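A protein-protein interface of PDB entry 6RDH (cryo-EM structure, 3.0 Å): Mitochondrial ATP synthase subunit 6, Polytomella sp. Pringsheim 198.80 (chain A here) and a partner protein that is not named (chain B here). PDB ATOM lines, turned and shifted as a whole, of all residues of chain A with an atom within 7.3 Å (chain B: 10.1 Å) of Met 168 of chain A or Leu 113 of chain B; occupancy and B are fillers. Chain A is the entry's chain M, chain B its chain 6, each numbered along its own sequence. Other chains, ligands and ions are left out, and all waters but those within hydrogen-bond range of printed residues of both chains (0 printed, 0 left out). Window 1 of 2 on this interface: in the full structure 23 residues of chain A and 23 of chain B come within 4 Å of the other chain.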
ATOM      1  N   SER A 161       7.697   2.899  -2.329  1.00  0.00           N
ATOM      2  CA  SER A 161       6.331   2.611  -1.913  1.00  0.00           C
ATOM      3  C   SER A 161       6.031   3.226  -0.552  1.00  0.00           C
ATOM      4  O   SER A 161       4.957   3.802  -0.353  1.00  0.00           O
ATOM      5  CB  SER A 161       6.091   1.109  -1.904  1.00  0.00           C
ATOM      6  OG  SER A 161       7.099   0.441  -1.181  1.00  0.00           O
ATOM      7  N   ASN A 163       7.469   5.909   0.582  1.00  0.00           N
ATOM      8  CA  ASN A 163       7.456   7.356   0.421  1.00  0.00           C
ATOM      9  C   ASN A 163       6.174   7.824  -0.237  1.00  0.00           C
ATOM     10  O   ASN A 163       5.655   8.886   0.107  1.00  0.00           O
ATOM     11  CB  ASN A 163       8.646   7.814  -0.410  1.00  0.00           C
ATOM     12  CG  ASN A 163       9.911   7.880   0.378  1.00  0.00           C
ATOM     13  OD1 ASN A 163      10.962   8.210  -0.151  1.00  0.00           O
ATOM     14  ND2 ASN A 163       9.829   7.557   1.650  1.00  0.00           N
ATOM     15  N   LEU A 164       5.659   7.058  -1.194  1.00  0.00           N
ATOM     16  CA  LEU A 164       4.413   7.418  -1.842  1.00  0.00           C
ATOM     17  C   LEU A 164       3.188   7.044  -1.030  1.00  0.00           C
ATOM     18  O   LEU A 164       2.090   7.464  -1.395  1.00  0.00           O
ATOM     19  CB  LEU A 164       4.328   6.766  -3.216  1.00  0.00           C
ATOM     20  CG  LEU A 164       5.297   7.282  -4.270  1.00  0.00           C
ATOM     21  CD1 LEU A 164       5.107   6.492  -5.531  1.00  0.00           C
ATOM     22  CD2 LEU A 164       5.088   8.743  -4.530  1.00  0.00           C
ATOM     23  N   LEU A 165       3.329   6.250   0.036  1.00  0.00           N
ATOM     24  CA  LEU A 165       2.215   6.119   0.970  1.00  0.00           C
ATOM     25  C   LEU A 165       1.907   7.428   1.665  1.00  0.00           C
ATOM     26  O   LEU A 165       0.746   7.705   1.962  1.00  0.00           O
ATOM     27  CB  LEU A 165       2.477   5.056   2.023  1.00  0.00           C
ATOM     28  CG  LEU A 165       2.233   3.627   1.607  1.00  0.00           C
ATOM     29  CD1 LEU A 165       2.580   2.712   2.749  1.00  0.00           C
ATOM     30  CD2 LEU A 165       0.784   3.507   1.249  1.00  0.00           C
ATOM     31  N   GLY A 166       2.909   8.258   1.900  1.00  0.00           N
ATOM     32  CA  GLY A 166       2.663   9.520   2.560  1.00  0.00           C
ATOM     33  C   GLY A 166       1.963  10.557   1.724  1.00  0.00           C
ATOM     34  O   GLY A 166       1.716  11.659   2.215  1.00  0.00           O
ATOM     35  N   LEU A 167       1.647  10.243   0.472  1.00  0.00           N
ATOM     36  CA  LEU A 167       0.961  11.139  -0.438  1.00  0.00           C
ATOM     37  C   LEU A 167      -0.399  10.617  -0.861  1.00  0.00           C
ATOM     38  O   LEU A 167      -1.078  11.273  -1.653  1.00  0.00           O
ATOM     39  CB  LEU A 167       1.828  11.383  -1.667  1.00  0.00           C
ATOM     40  CG  LEU A 167       3.164  11.974  -1.257  1.00  0.00           C
ATOM     41  CD1 LEU A 167       4.160  11.771  -2.334  1.00  0.00           C
ATOM     42  CD2 LEU A 167       2.972  13.429  -0.950  1.00  0.00           C
ATOM     43  N   MET A 168      -0.776   9.494  -0.407  1.00  0.00           N
ATOM     44  CA  MET A 168      -2.142   9.023  -0.512  1.00  0.00           C
ATOM     45  C   MET A 168      -2.946   9.562   0.659  1.00  0.00           C
ATOM     46  O   MET A 168      -2.393   9.787   1.735  1.00  0.00           O
ATOM     47  CB  MET A 168      -2.186   7.503  -0.504  1.00  0.00           C
ATOM     48  CG  MET A 168      -1.340   6.856  -1.571  1.00  0.00           C
ATOM     49  SD  MET A 168      -1.908   7.232  -3.229  1.00  0.00           S
ATOM     50  CE  MET A 168      -0.519   8.157  -3.869  1.00  0.00           C
ATOM     51  N   PRO A 169      -4.237   9.820   0.482  1.00  0.00           N
ATOM     52  CA  PRO A 169      -5.049  10.293   1.603  1.00  0.00           C
ATOM     53  C   PRO A 169      -5.220   9.231   2.673  1.00  0.00           C
ATOM     54  O   PRO A 169      -5.092   8.033   2.422  1.00  0.00           O
ATOM     55  CB  PRO A 169      -6.385  10.645   0.949  1.00  0.00           C
ATOM     56  CG  PRO A 169      -6.359  10.001  -0.367  1.00  0.00           C
ATOM     57  CD  PRO A 169      -4.949   9.971  -0.792  1.00  0.00           C
ATOM     58  N   PHE A 170      -5.463   9.716   3.892  1.00  0.00           N
ATOM     59  CA  PHE A 170      -5.626   8.919   5.109  1.00  0.00           C
ATOM     60  C   PHE A 170      -4.399   8.082   5.434  1.00  0.00           C
ATOM     61  O   PHE A 170      -4.499   7.079   6.134  1.00  0.00           O
ATOM     62  CB  PHE A 170      -6.865   8.025   5.047  1.00  0.00           C
ATOM     63  CG  PHE A 170      -8.120   8.761   4.725  1.00  0.00           C
ATOM     64  CD1 PHE A 170      -8.801   9.450   5.705  1.00  0.00           C
ATOM     65  CD2 PHE A 170      -8.625   8.758   3.444  1.00  0.00           C
ATOM     66  CE1 PHE A 170      -9.951  10.125   5.411  1.00  0.00           C
ATOM     67  CE2 PHE A 170      -9.774   9.435   3.146  1.00  0.00           C
ATOM     68  CZ  PHE A 170     -10.435  10.117   4.130  1.00  0.00           C
ATOM     69  N   ASN A 171      -3.222   8.495   4.979  1.00  0.00           N
ATOM     70  CA  ASN A 171      -2.049   7.660   5.158  1.00  0.00           C
ATOM     71  C   ASN A 171      -0.847   8.511   5.512  1.00  0.00           C
ATOM     72  O   ASN A 171      -0.728   9.662   5.090  1.00  0.00           O
ATOM     73  CB  ASN A 171      -1.741   6.839   3.913  1.00  0.00           C
ATOM     74  CG  ASN A 171      -2.455   5.528   3.904  1.00  0.00           C
ATOM     75  OD1 ASN A 171      -2.144   4.642   4.689  1.00  0.00           O
ATOM     76  ND2 ASN A 171      -3.417   5.385   3.013  1.00  0.00           N
ATOM     77  N   GLU A 172       0.032   7.923   6.308  1.00  0.00           N
ATOM     78  CA  GLU A 172       1.327   8.479   6.643  1.00  0.00           C
ATOM     79  C   GLU A 172       2.394   7.622   5.990  1.00  0.00           C
ATOM     80  O   GLU A 172       2.191   6.431   5.752  1.00  0.00           O
ATOM     81  CB  GLU A 172       1.533   8.515   8.158  1.00  0.00           C
ATOM     82  CG  GLU A 172       2.846   9.157   8.558  1.00  0.00           C
ATOM     83  CD  GLU A 172       3.050   9.248  10.053  1.00  0.00           C
ATOM     84  OE1 GLU A 172       2.174   8.771  10.802  1.00  0.00           O
ATOM     85  OE2 GLU A 172       4.096   9.787  10.477  1.00  0.00           O
ATOM     86  N   ALA A 173       3.514   8.241   5.667  1.00  0.00           N
ATOM     87  CA  ALA A 173       4.634   7.493   5.137  1.00  0.00           C
ATOM     88  C   ALA A 173       5.266   6.668   6.251  1.00  0.00           C
ATOM     89  O   ALA A 173       5.441   7.167   7.365  1.00  0.00           O
ATOM     90  CB  ALA A 173       5.665   8.438   4.538  1.00  0.00           C
ATOM     91  N   TYR A 289       5.811  15.164  -3.803  1.00  0.00           N
ATOM     92  CA  TYR A 289       5.889  14.058  -4.759  1.00  0.00           C
ATOM     93  C   TYR A 289       7.280  13.947  -5.364  1.00  0.00           C
ATOM     94  O   TYR A 289       7.840  12.843  -5.480  1.00  0.00           O
ATOM     95  CB  TYR A 289       4.865  14.246  -5.868  1.00  0.00           C
ATOM     96  CG  TYR A 289       3.529  13.640  -5.572  1.00  0.00           C
ATOM     97  CD1 TYR A 289       3.286  12.308  -5.825  1.00  0.00           C
ATOM     98  CD2 TYR A 289       2.512  14.402  -5.043  1.00  0.00           C
ATOM     99  CE1 TYR A 289       2.069  11.754  -5.551  1.00  0.00           C
ATOM    100  CE2 TYR A 289       1.297  13.859  -4.766  1.00  0.00           C
ATOM    101  CZ  TYR A 289       1.076  12.536  -5.029  1.00  0.00           C
ATOM    102  OH  TYR A 289      -0.147  11.992  -4.747  1.00  0.00           O
ATOM    103  N   TRP B  85      -9.451   0.130   6.234  1.00  0.00           N
ATOM    104  CA  TRP B  85      -8.267   0.913   6.548  1.00  0.00           C
ATOM    105  C   TRP B  85      -8.556   2.399   6.463  1.00  0.00           C
ATOM    106  O   TRP B  85      -8.101   3.163   7.313  1.00  0.00           O
ATOM    107  CB  TRP B  85      -7.133   0.535   5.603  1.00  0.00           C
ATOM    108  CG  TRP B  85      -5.876   1.270   5.848  1.00  0.00           C
ATOM    109  CD1 TRP B  85      -5.384   2.313   5.134  1.00  0.00           C
ATOM    110  CD2 TRP B  85      -4.936   1.013   6.883  1.00  0.00           C
ATOM    111  NE1 TRP B  85      -4.195   2.725   5.661  1.00  0.00           N
ATOM    112  CE2 TRP B  85      -3.899   1.938   6.739  1.00  0.00           C
ATOM    113  CE3 TRP B  85      -4.873   0.088   7.920  1.00  0.00           C
ATOM    114  CZ2 TRP B  85      -2.816   1.968   7.595  1.00  0.00           C
ATOM    115  CZ3 TRP B  85      -3.800   0.122   8.763  1.00  0.00           C
ATOM    116  CH2 TRP B  85      -2.785   1.049   8.598  1.00  0.00           C
ATOM    117  N   ILE B  86      -9.328   2.824   5.463  1.00  0.00           N
ATOM    118  CA  ILE B  86      -9.647   4.240   5.322  1.00  0.00           C
ATOM    119  C   ILE B  86     -10.534   4.705   6.469  1.00  0.00           C
ATOM    120  O   ILE B  86     -10.315   5.778   7.040  1.00  0.00           O
ATOM    121  CB  ILE B  86     -10.284   4.491   3.946  1.00  0.00           C
ATOM    122  CG1 ILE B  86      -9.207   4.450   2.868  1.00  0.00           C
ATOM    123  CG2 ILE B  86     -10.997   5.817   3.893  1.00  0.00           C
ATOM    124  CD1 ILE B  86      -9.757   4.473   1.472  1.00  0.00           C
ATOM    125  N   ARG B  89      -8.248   4.741   9.710  1.00  0.00           N
ATOM    126  CA  ARG B  89      -7.341   5.878   9.669  1.00  0.00           C
ATOM    127  C   ARG B  89      -8.082   7.198   9.788  1.00  0.00           C
ATOM    128  O   ARG B  89      -7.528   8.158  10.316  1.00  0.00           O
ATOM    129  CB  ARG B  89      -6.530   5.852   8.382  1.00  0.00           C
ATOM    130  CG  ARG B  89      -5.513   4.754   8.315  1.00  0.00           C
ATOM    131  CD  ARG B  89      -4.343   5.034   9.187  1.00  0.00           C
ATOM    132  NE  ARG B  89      -3.803   6.353   8.922  1.00  0.00           N
ATOM    133  CZ  ARG B  89      -2.605   6.742   9.318  1.00  0.00           C
ATOM    134  NH1 ARG B  89      -1.832   5.903   9.982  1.00  0.00           N
ATOM    135  NH2 ARG B  89      -2.184   7.964   9.051  1.00  0.00           N
ATOM    136  N   GLN B  93      -7.466   9.893  12.615  1.00  0.00           N
ATOM    137  CA  GLN B  93      -7.072  11.251  12.261  1.00  0.00           C
ATOM    138  C   GLN B  93      -7.950  12.275  12.939  1.00  0.00           C
ATOM    139  O   GLN B  93      -7.497  13.380  13.248  1.00  0.00           O
ATOM    140  CB  GLN B  93      -7.136  11.474  10.755  1.00  0.00           C
ATOM    141  CG  GLN B  93      -5.969  10.964   9.980  1.00  0.00           C
ATOM    142  CD  GLN B  93      -6.100  11.289   8.526  1.00  0.00           C
ATOM    143  OE1 GLN B  93      -7.134  11.765   8.081  1.00  0.00           O
ATOM    144  NE2 GLN B  93      -5.031  11.076   7.777  1.00  0.00           N
ATOM    145  N   ASP B 102      -5.434  17.373   9.772  1.00  0.00           N
ATOM    146  CA  ASP B 102      -5.313  16.068   9.122  1.00  0.00           C
ATOM    147  C   ASP B 102      -6.421  15.838   8.105  1.00  0.00           C
ATOM    148  O   ASP B 102      -6.163  15.334   6.999  1.00  0.00           O
ATOM    149  CB  ASP B 102      -5.336  14.950  10.157  1.00  0.00           C
ATOM    150  CG  ASP B 102      -4.174  15.014  11.106  1.00  0.00           C
ATOM    151  OD1 ASP B 102      -3.504  16.059  11.138  1.00  0.00           O
ATOM    152  OD2 ASP B 102      -3.921  14.020  11.815  1.00  0.00           O
ATOM    153  N   ASN B 104      -7.950  18.029   6.425  1.00  0.00           N
ATOM    154  CA  ASN B 104      -7.682  18.845   5.254  1.00  0.00           C
ATOM    155  C   ASN B 104      -6.426  18.426   4.505  1.00  0.00           C
ATOM    156  O   ASN B 104      -6.304  18.717   3.312  1.00  0.00           O
ATOM    157  CB  ASN B 104      -7.616  20.295   5.691  1.00  0.00           C
ATOM    158  CG  ASN B 104      -8.975  20.830   6.037  1.00  0.00           C
ATOM    159  OD1 ASN B 104      -9.689  20.279   6.861  1.00  0.00           O
ATOM    160  ND2 ASN B 104      -9.336  21.910   5.421  1.00  0.00           N
ATOM    161  N   LEU B 105      -5.505  17.724   5.160  1.00  0.00           N
ATOM    162  CA  LEU B 105      -4.385  17.149   4.427  1.00  0.00           C
ATOM    163  C   LEU B 105      -4.829  16.000   3.542  1.00  0.00           C
ATOM    164  O   LEU B 105      -4.234  15.776   2.482  1.00  0.00           O
ATOM    165  CB  LEU B 105      -3.307  16.688   5.393  1.00  0.00           C
ATOM    166  CG  LEU B 105      -2.394  17.818   5.843  1.00  0.00           C
ATOM    167  CD1 LEU B 105      -1.308  17.278   6.722  1.00  0.00           C
ATOM    168  CD2 LEU B 105      -1.802  18.498   4.652  1.00  0.00           C
ATOM    169  N   ASN B 106      -5.867  15.271   3.954  1.00  0.00           N
ATOM    170  CA  ASN B 106      -6.456  14.269   3.067  1.00  0.00           C
ATOM    171  C   ASN B 106      -7.022  14.909   1.803  1.00  0.00           C
ATOM    172  O   ASN B 106      -6.911  14.346   0.710  1.00  0.00           O
ATOM    173  CB  ASN B 106      -7.543  13.492   3.793  1.00  0.00           C
ATOM    174  CG  ASN B 106      -7.027  12.782   5.002  1.00  0.00           C
ATOM    175  OD1 ASN B 106      -5.879  12.361   5.042  1.00  0.00           O
ATOM    176  ND2 ASN B 106      -7.870  12.648   6.007  1.00  0.00           N
ATOM    177  N   VAL B 107      -7.595  16.103   1.929  1.00  0.00           N
ATOM    178  CA  VAL B 107      -8.082  16.843   0.771  1.00  0.00           C
ATOM    179  C   VAL B 107      -6.922  17.311  -0.093  1.00  0.00           C
ATOM    180  O   VAL B 107      -6.971  17.219  -1.324  1.00  0.00           O
ATOM    181  CB  VAL B 107      -8.955  18.016   1.245  1.00  0.00           C
ATOM    182  CG1 VAL B 107      -9.254  18.974   0.123  1.00  0.00           C
ATOM    183  CG2 VAL B 107     -10.238  17.495   1.830  1.00  0.00           C
ATOM    184  N   LEU B 108      -5.849  17.787   0.543  1.00  0.00           N
ATOM    185  CA  LEU B 108      -4.682  18.270  -0.190  1.00  0.00           C
ATOM    186  C   LEU B 108      -3.982  17.161  -0.954  1.00  0.00           C
ATOM    187  O   LEU B 108      -3.350  17.420  -1.979  1.00  0.00           O
ATOM    188  CB  LEU B 108      -3.701  18.922   0.768  1.00  0.00           C
ATOM    189  CG  LEU B 108      -3.878  20.420   0.898  1.00  0.00           C
ATOM    190  CD1 LEU B 108      -2.952  20.911   1.953  1.00  0.00           C
ATOM    191  CD2 LEU B 108      -3.561  21.070  -0.419  1.00  0.00           C
ATOM    192  N   GLN B 109      -4.082  15.928  -0.477  1.00  0.00           N
ATOM    193  CA  GLN B 109      -3.500  14.801  -1.189  1.00  0.00           C
ATOM    194  C   GLN B 109      -4.423  14.233  -2.265  1.00  0.00           C
ATOM    195  O   GLN B 109      -3.962  13.893  -3.365  1.00  0.00           O
ATOM    196  CB  GLN B 109      -3.117  13.725  -0.182  1.00  0.00           C
ATOM    197  CG  GLN B 109      -1.975  14.165   0.684  1.00  0.00           C
ATOM    198  CD  GLN B 109      -1.912  13.428   1.977  1.00  0.00           C
ATOM    199  OE1 GLN B 109      -2.789  12.642   2.293  1.00  0.00           O
ATOM    200  NE2 GLN B 109      -0.866  13.677   2.741  1.00  0.00           N
ATOM    201  N   ALA B 110      -5.726  14.133  -1.977  1.00  0.00           N
ATOM    202  CA  ALA B 110      -6.671  13.665  -2.981  1.00  0.00           C
ATOM    203  C   ALA B 110      -6.792  14.640  -4.140  1.00  0.00           C
ATOM    204  O   ALA B 110      -7.126  14.234  -5.257  1.00  0.00           O
ATOM    205  CB  ALA B 110      -8.033  13.430  -2.344  1.00  0.00           C
ATOM    206  N   ALA B 111      -6.496  15.919  -3.902  1.00  0.00           N
ATOM    207  CA  ALA B 111      -6.456  16.890  -4.986  1.00  0.00           C
ATOM    208  C   ALA B 111      -5.352  16.564  -5.975  1.00  0.00           C
ATOM    209  O   ALA B 111      -5.540  16.697  -7.186  1.00  0.00           O
ATOM    210  CB  ALA B 111      -6.268  18.290  -4.420  1.00  0.00           C
ATOM    211  N   TRP B 112      -4.204  16.101  -5.488  1.00  0.00           N
ATOM    212  CA  TRP B 112      -3.119  15.764  -6.404  1.00  0.00           C
ATOM    213  C   TRP B 112      -3.327  14.418  -7.057  1.00  0.00           C
ATOM    214  O   TRP B 112      -2.829  14.198  -8.158  1.00  0.00           O
ATOM    215  CB  TRP B 112      -1.781  15.767  -5.689  1.00  0.00           C
ATOM    216  CG  TRP B 112      -1.085  17.029  -5.822  1.00  0.00           C
ATOM    217  CD1 TRP B 112      -0.972  17.980  -4.883  1.00  0.00           C
ATOM    218  CD2 TRP B 112      -0.423  17.523  -6.981  1.00  0.00           C
ATOM    219  NE1 TRP B 112      -0.258  19.041  -5.362  1.00  0.00           N
ATOM    220  CE2 TRP B 112       0.088  18.783  -6.657  1.00  0.00           C
ATOM    221  CE3 TRP B 112      -0.212  17.022  -8.262  1.00  0.00           C
ATOM    222  CZ2 TRP B 112       0.800  19.551  -7.560  1.00  0.00           C
ATOM    223  CZ3 TRP B 112       0.498  17.781  -9.157  1.00  0.00           C
ATOM    224  CH2 TRP B 112       0.997  19.033  -8.805  1.00  0.00           C
ATOM    225  N   LEU B 113      -4.042  13.511  -6.396  1.00  0.00           N
ATOM    226  CA  LEU B 113      -4.482  12.291  -7.075  1.00  0.00           C
ATOM    227  C   LEU B 113      -5.404  12.619  -8.245  1.00  0.00           C
ATOM    228  O   LEU B 113      -5.246  12.077  -9.347  1.00  0.00           O
ATOM    229  CB  LEU B 113      -5.193  11.373  -6.088  1.00  0.00           C
ATOM    230  CG  LEU B 113      -4.432  10.203  -5.487  1.00  0.00           C
ATOM    231  CD1 LEU B 113      -3.277  10.693  -4.683  1.00  0.00           C
ATOM    232  CD2 LEU B 113      -5.357   9.398  -4.619  1.00  0.00           C
ATOM    233  N   ILE B 114      -6.354  13.530  -8.022  1.00  0.00           N
ATOM    234  CA  ILE B 114      -7.266  13.984  -9.071  1.00  0.00           C
ATOM    235  C   ILE B 114      -6.503  14.707 -10.178  1.00  0.00           C
ATOM    236  O   ILE B 114      -6.795  14.538 -11.366  1.00  0.00           O
ATOM    237  CB  ILE B 114      -8.357  14.867  -8.430  1.00  0.00           C
ATOM    238  CG1 ILE B 114      -9.395  13.999  -7.735  1.00  0.00           C
ATOM    239  CG2 ILE B 114      -9.024  15.794  -9.416  1.00  0.00           C
ATOM    240  CD1 ILE B 114     -10.396  14.786  -6.961  1.00  0.00           C
ATOM    241  N   SER B 115      -5.490  15.486  -9.811  1.00  0.00           N
ATOM    242  CA  SER B 115      -4.699  16.199 -10.803  1.00  0.00           C
ATOM    243  C   SER B 115      -3.794  15.274 -11.603  1.00  0.00           C
ATOM    244  O   SER B 115      -3.572  15.520 -12.789  1.00  0.00           O
ATOM    245  CB  SER B 115      -3.861  17.272 -10.126  1.00  0.00           C
ATOM    246  OG  SER B 115      -3.041  17.932 -11.066  1.00  0.00           O
ATOM    247  N   PHE B 116      -3.267  14.219 -10.985  1.00  0.00           N
ATOM    248  CA  PHE B 116      -2.467  13.251 -11.718  1.00  0.00           C
ATOM    249  C   PHE B 116      -3.312  12.399 -12.637  1.00  0.00           C
ATOM    250  O   PHE B 116      -2.850  12.016 -13.710  1.00  0.00           O
ATOM    251  CB  PHE B 116      -1.689  12.366 -10.757  1.00  0.00           C
ATOM    252  CG  PHE B 116      -0.428  12.981 -10.269  1.00  0.00           C
ATOM    253  CD1 PHE B 116       0.169  14.002 -10.978  1.00  0.00           C
ATOM    254  CD2 PHE B 116       0.160  12.547  -9.111  1.00  0.00           C
ATOM    255  CE1 PHE B 116       1.330  14.574 -10.542  1.00  0.00           C
ATOM    256  CE2 PHE B 116       1.312  13.122  -8.674  1.00  0.00           C
ATOM    257  CZ  PHE B 116       1.900  14.136  -9.390  1.00  0.00           C
ATOM    258  N   SER B 117      -4.559  12.125 -12.277  1.00  0.00           N
ATOM    259  CA  SER B 117      -5.399  11.383 -13.208  1.00  0.00           C
ATOM    260  C   SER B 117      -5.970  12.245 -14.327  1.00  0.00           C
ATOM    261  O   SER B 117      -6.889  11.797 -15.010  1.00  0.00           O
ATOM    262  CB  SER B 117      -6.543  10.701 -12.470  1.00  0.00           C
ATOM    263  OG  SER B 117      -7.440  11.659 -11.956  1.00  0.00           O
ATOM    264  N   SER B 118      -5.470  13.463 -14.523  1.00  0.00           N
ATOM    265  CA  SER B 118      -6.021  14.378 -15.501  1.00  0.00           C
ATOM    266  C   SER B 118      -4.989  15.011 -16.418  1.00  0.00           C
ATOM    267  O   SER B 118      -5.357  15.469 -17.500  1.00  0.00           O
ATOM    268  CB  SER B 118      -6.788  15.500 -14.791  1.00  0.00           C
ATOM    269  OG  SER B 118      -7.230  16.467 -15.717  1.00  0.00           O
ATOM    270  N   LEU B 119      -3.715  15.049 -16.032  1.00  0.00           N
ATOM    271  CA  LEU B 119      -2.696  15.629 -16.891  1.00  0.00           C
ATOM    272  C   LEU B 119      -1.570  14.674 -17.253  1.00  0.00           C
ATOM    273  O   LEU B 119      -0.757  15.012 -18.117  1.00  0.00           O
ATOM    274  CB  LEU B 119      -2.124  16.903 -16.254  1.00  0.00           C
ATOM    275  CG  LEU B 119      -1.477  16.920 -14.871  1.00  0.00           C
ATOM    276  CD1 LEU B 119       0.031  16.674 -14.873  1.00  0.00           C
ATOM    277  CD2 LEU B 119      -1.805  18.241 -14.209  1.00  0.00           C
ATOM    278  N   ILE B 120      -1.491  13.514 -16.615  1.00  0.00           N
ATOM    279  CA  ILE B 120      -0.522  12.490 -17.023  1.00  0.00           C
ATOM    280  C   ILE B 120      -0.953  11.908 -18.365  1.00  0.00           C
ATOM    281  O   ILE B 120      -2.114  11.495 -18.507  1.00  0.00           O
ATOM    282  CB  ILE B 120      -0.421  11.396 -15.962  1.00  0.00           C
ATOM    283  CG1 ILE B 120       0.267  11.922 -14.710  1.00  0.00           C
ATOM    284  CG2 ILE B 120       0.345  10.211 -16.477  1.00  0.00           C
ATOM    285  CD1 ILE B 120       0.376  10.896 -13.608  1.00  0.00           C
ATOM    286  N   PHE B 122      -1.322   8.927 -20.452  1.00  0.00           N
ATOM    287  CA  PHE B 122      -1.228   7.520 -20.094  1.00  0.00           C
ATOM    288  C   PHE B 122      -0.806   6.646 -21.260  1.00  0.00           C
ATOM    289  O   PHE B 122      -0.218   5.585 -21.043  1.00  0.00           O
ATOM    290  CB  PHE B 122      -2.547   7.045 -19.513  1.00  0.00           C
ATOM    291  CG  PHE B 122      -2.800   7.570 -18.148  1.00  0.00           C
ATOM    292  CD1 PHE B 122      -2.024   7.156 -17.089  1.00  0.00           C
ATOM    293  CD2 PHE B 122      -3.793   8.502 -17.925  1.00  0.00           C
ATOM    294  CE1 PHE B 122      -2.239   7.648 -15.831  1.00  0.00           C
ATOM    295  CE2 PHE B 122      -4.015   8.996 -16.666  1.00  0.00           C
ATOM    296  CZ  PHE B 122      -3.235   8.566 -15.618  1.00  0.00           C
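The backbone carbonyl oxygen of Gly 166 of chain A is in hydrogen-bond range of the side-chain amide nitrogen of Gln 109 of chain B, at 3.3 Å. O of Met 168 of chain A sits close to OE1 of Gln 109 of chain B (2.9 Å). The guanidinium group (NE) of Arg 89 of chain B is in hydrogen-bond range of the backbone carbonyl oxygen (O) of Phe 170 of chain A (3.0 Å). OD1 of Asn 106 of chain B is in hydrogen-bond range of N of Phe 170 of chain A (2.9 Å). The indole nitrogen of Trp 85 of chain B sits at hydrogen-bond distance from the side-chain amide oxygen of Asn 171 of chain A, at 3.0 Å.
O of Leu 167 of chain A lies within hydrogen-bond range of OH of Tyr 289 of chain A (3.3 Å). O of Pro 169 of chain A sits at hydrogen-bond distance from ND2 of Asn 171 of chain A (3.2 Å). NE2 of Gln 93 of chain B is in hydrogen-bond range of OD1 of Asn 106 of chain B, at 3.1 Å. ND2 of Asn 106 of chain B is in hydrogen-bond range of O of Asp 102 of chain B (3.3 Å). O of Leu 105 of chain B sits close to OE1 of Gln 109 of chain B (3.5 Å). The backbone carbonyl oxygen (O) of Leu 113 of chain B is in hydrogen-bond range of the side-chain hydroxyl (OG) of Ser 117 of chain B, 3.4 Å away.
Among the printed residues, pairs that only touch across the chains: Leu 167 of chain A with Gln 109 of chain B (3.5 Å), Leu 167 of chain A with Leu 113 of chain B (3.8 Å), Met 168 of chain A with Leu 113 of chain B (3.8 Å), Pro 169 of chain A with Asn 106 of chain B (3.7 Å), Pro 169 of chain A with Gln 109 of chain B (3.3 Å), Pro 169 of chain A with Leu 113 of chain B (3.9 Å), Phe 170 of chain A with Ile 86 of chain B (3.8 Å), Phe 170 of chain A with Gln 93 of chain B (3.5 Å), Asn 171 of chain A with Arg 89 of chain B (3.8 Å), Glu 172 of chain A with Arg 89 of chain B (3.5 Å), Tyr 289 of chain A with Trp 112 of chain B (3.7 Å), Tyr 289 of chain A with Leu 113 of chain B (3.4 Å) and Tyr 289 of chain A with Phe 116 of chain B (3.5 Å).
Printed residues of chain B within 4 Å of Gly 166 of chain A: Gln 109. Leu 167 of chain A touches just these residues of chain B: Gln 109 and Leu 113. Of chain B, only Asn 106 (3.7 Å), Gln 109 (3.3 Å) and Leu 113 (3.9 Å) come within 4 Å of Pro 169 of chain A. Asn 171 of chain A touches two residues of chain B. Printed residues of chain A within 4 Å of Arg 89 of chain B: Phe 170, Asn 171 and Glu 172. Printed residues of chain A within 4 Å of Asn 106 of chain B: Pro 169 (3.7 Å) and Phe 170 (2.9 Å). The nearest residue of chain A that does not touch Leu 113 of chain B is Leu 164 of chain A (7.1 Å). The nearest printed residue of chain B that does not touch Tyr 289 of chain A is Gln 109 of chain B (4.5 Å).
Hydrophobic or aromatic side chains of chain B that line the printed part of chain A: Trp 85, Ile 86, Trp 112, Leu 113 and Phe 116. Hydrophobic or aromatic side chains of chain A within 4 Å of the printed part of chain B: Met 168, Pro 169, Phe 170 and Tyr 289. Among the printed residues, 18 pairs touch across the chains. Among the printed residues, no Asp or Glu carboxylate lies within 4 Å of a Lys or Arg side-chain nitrogen of the other chain.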
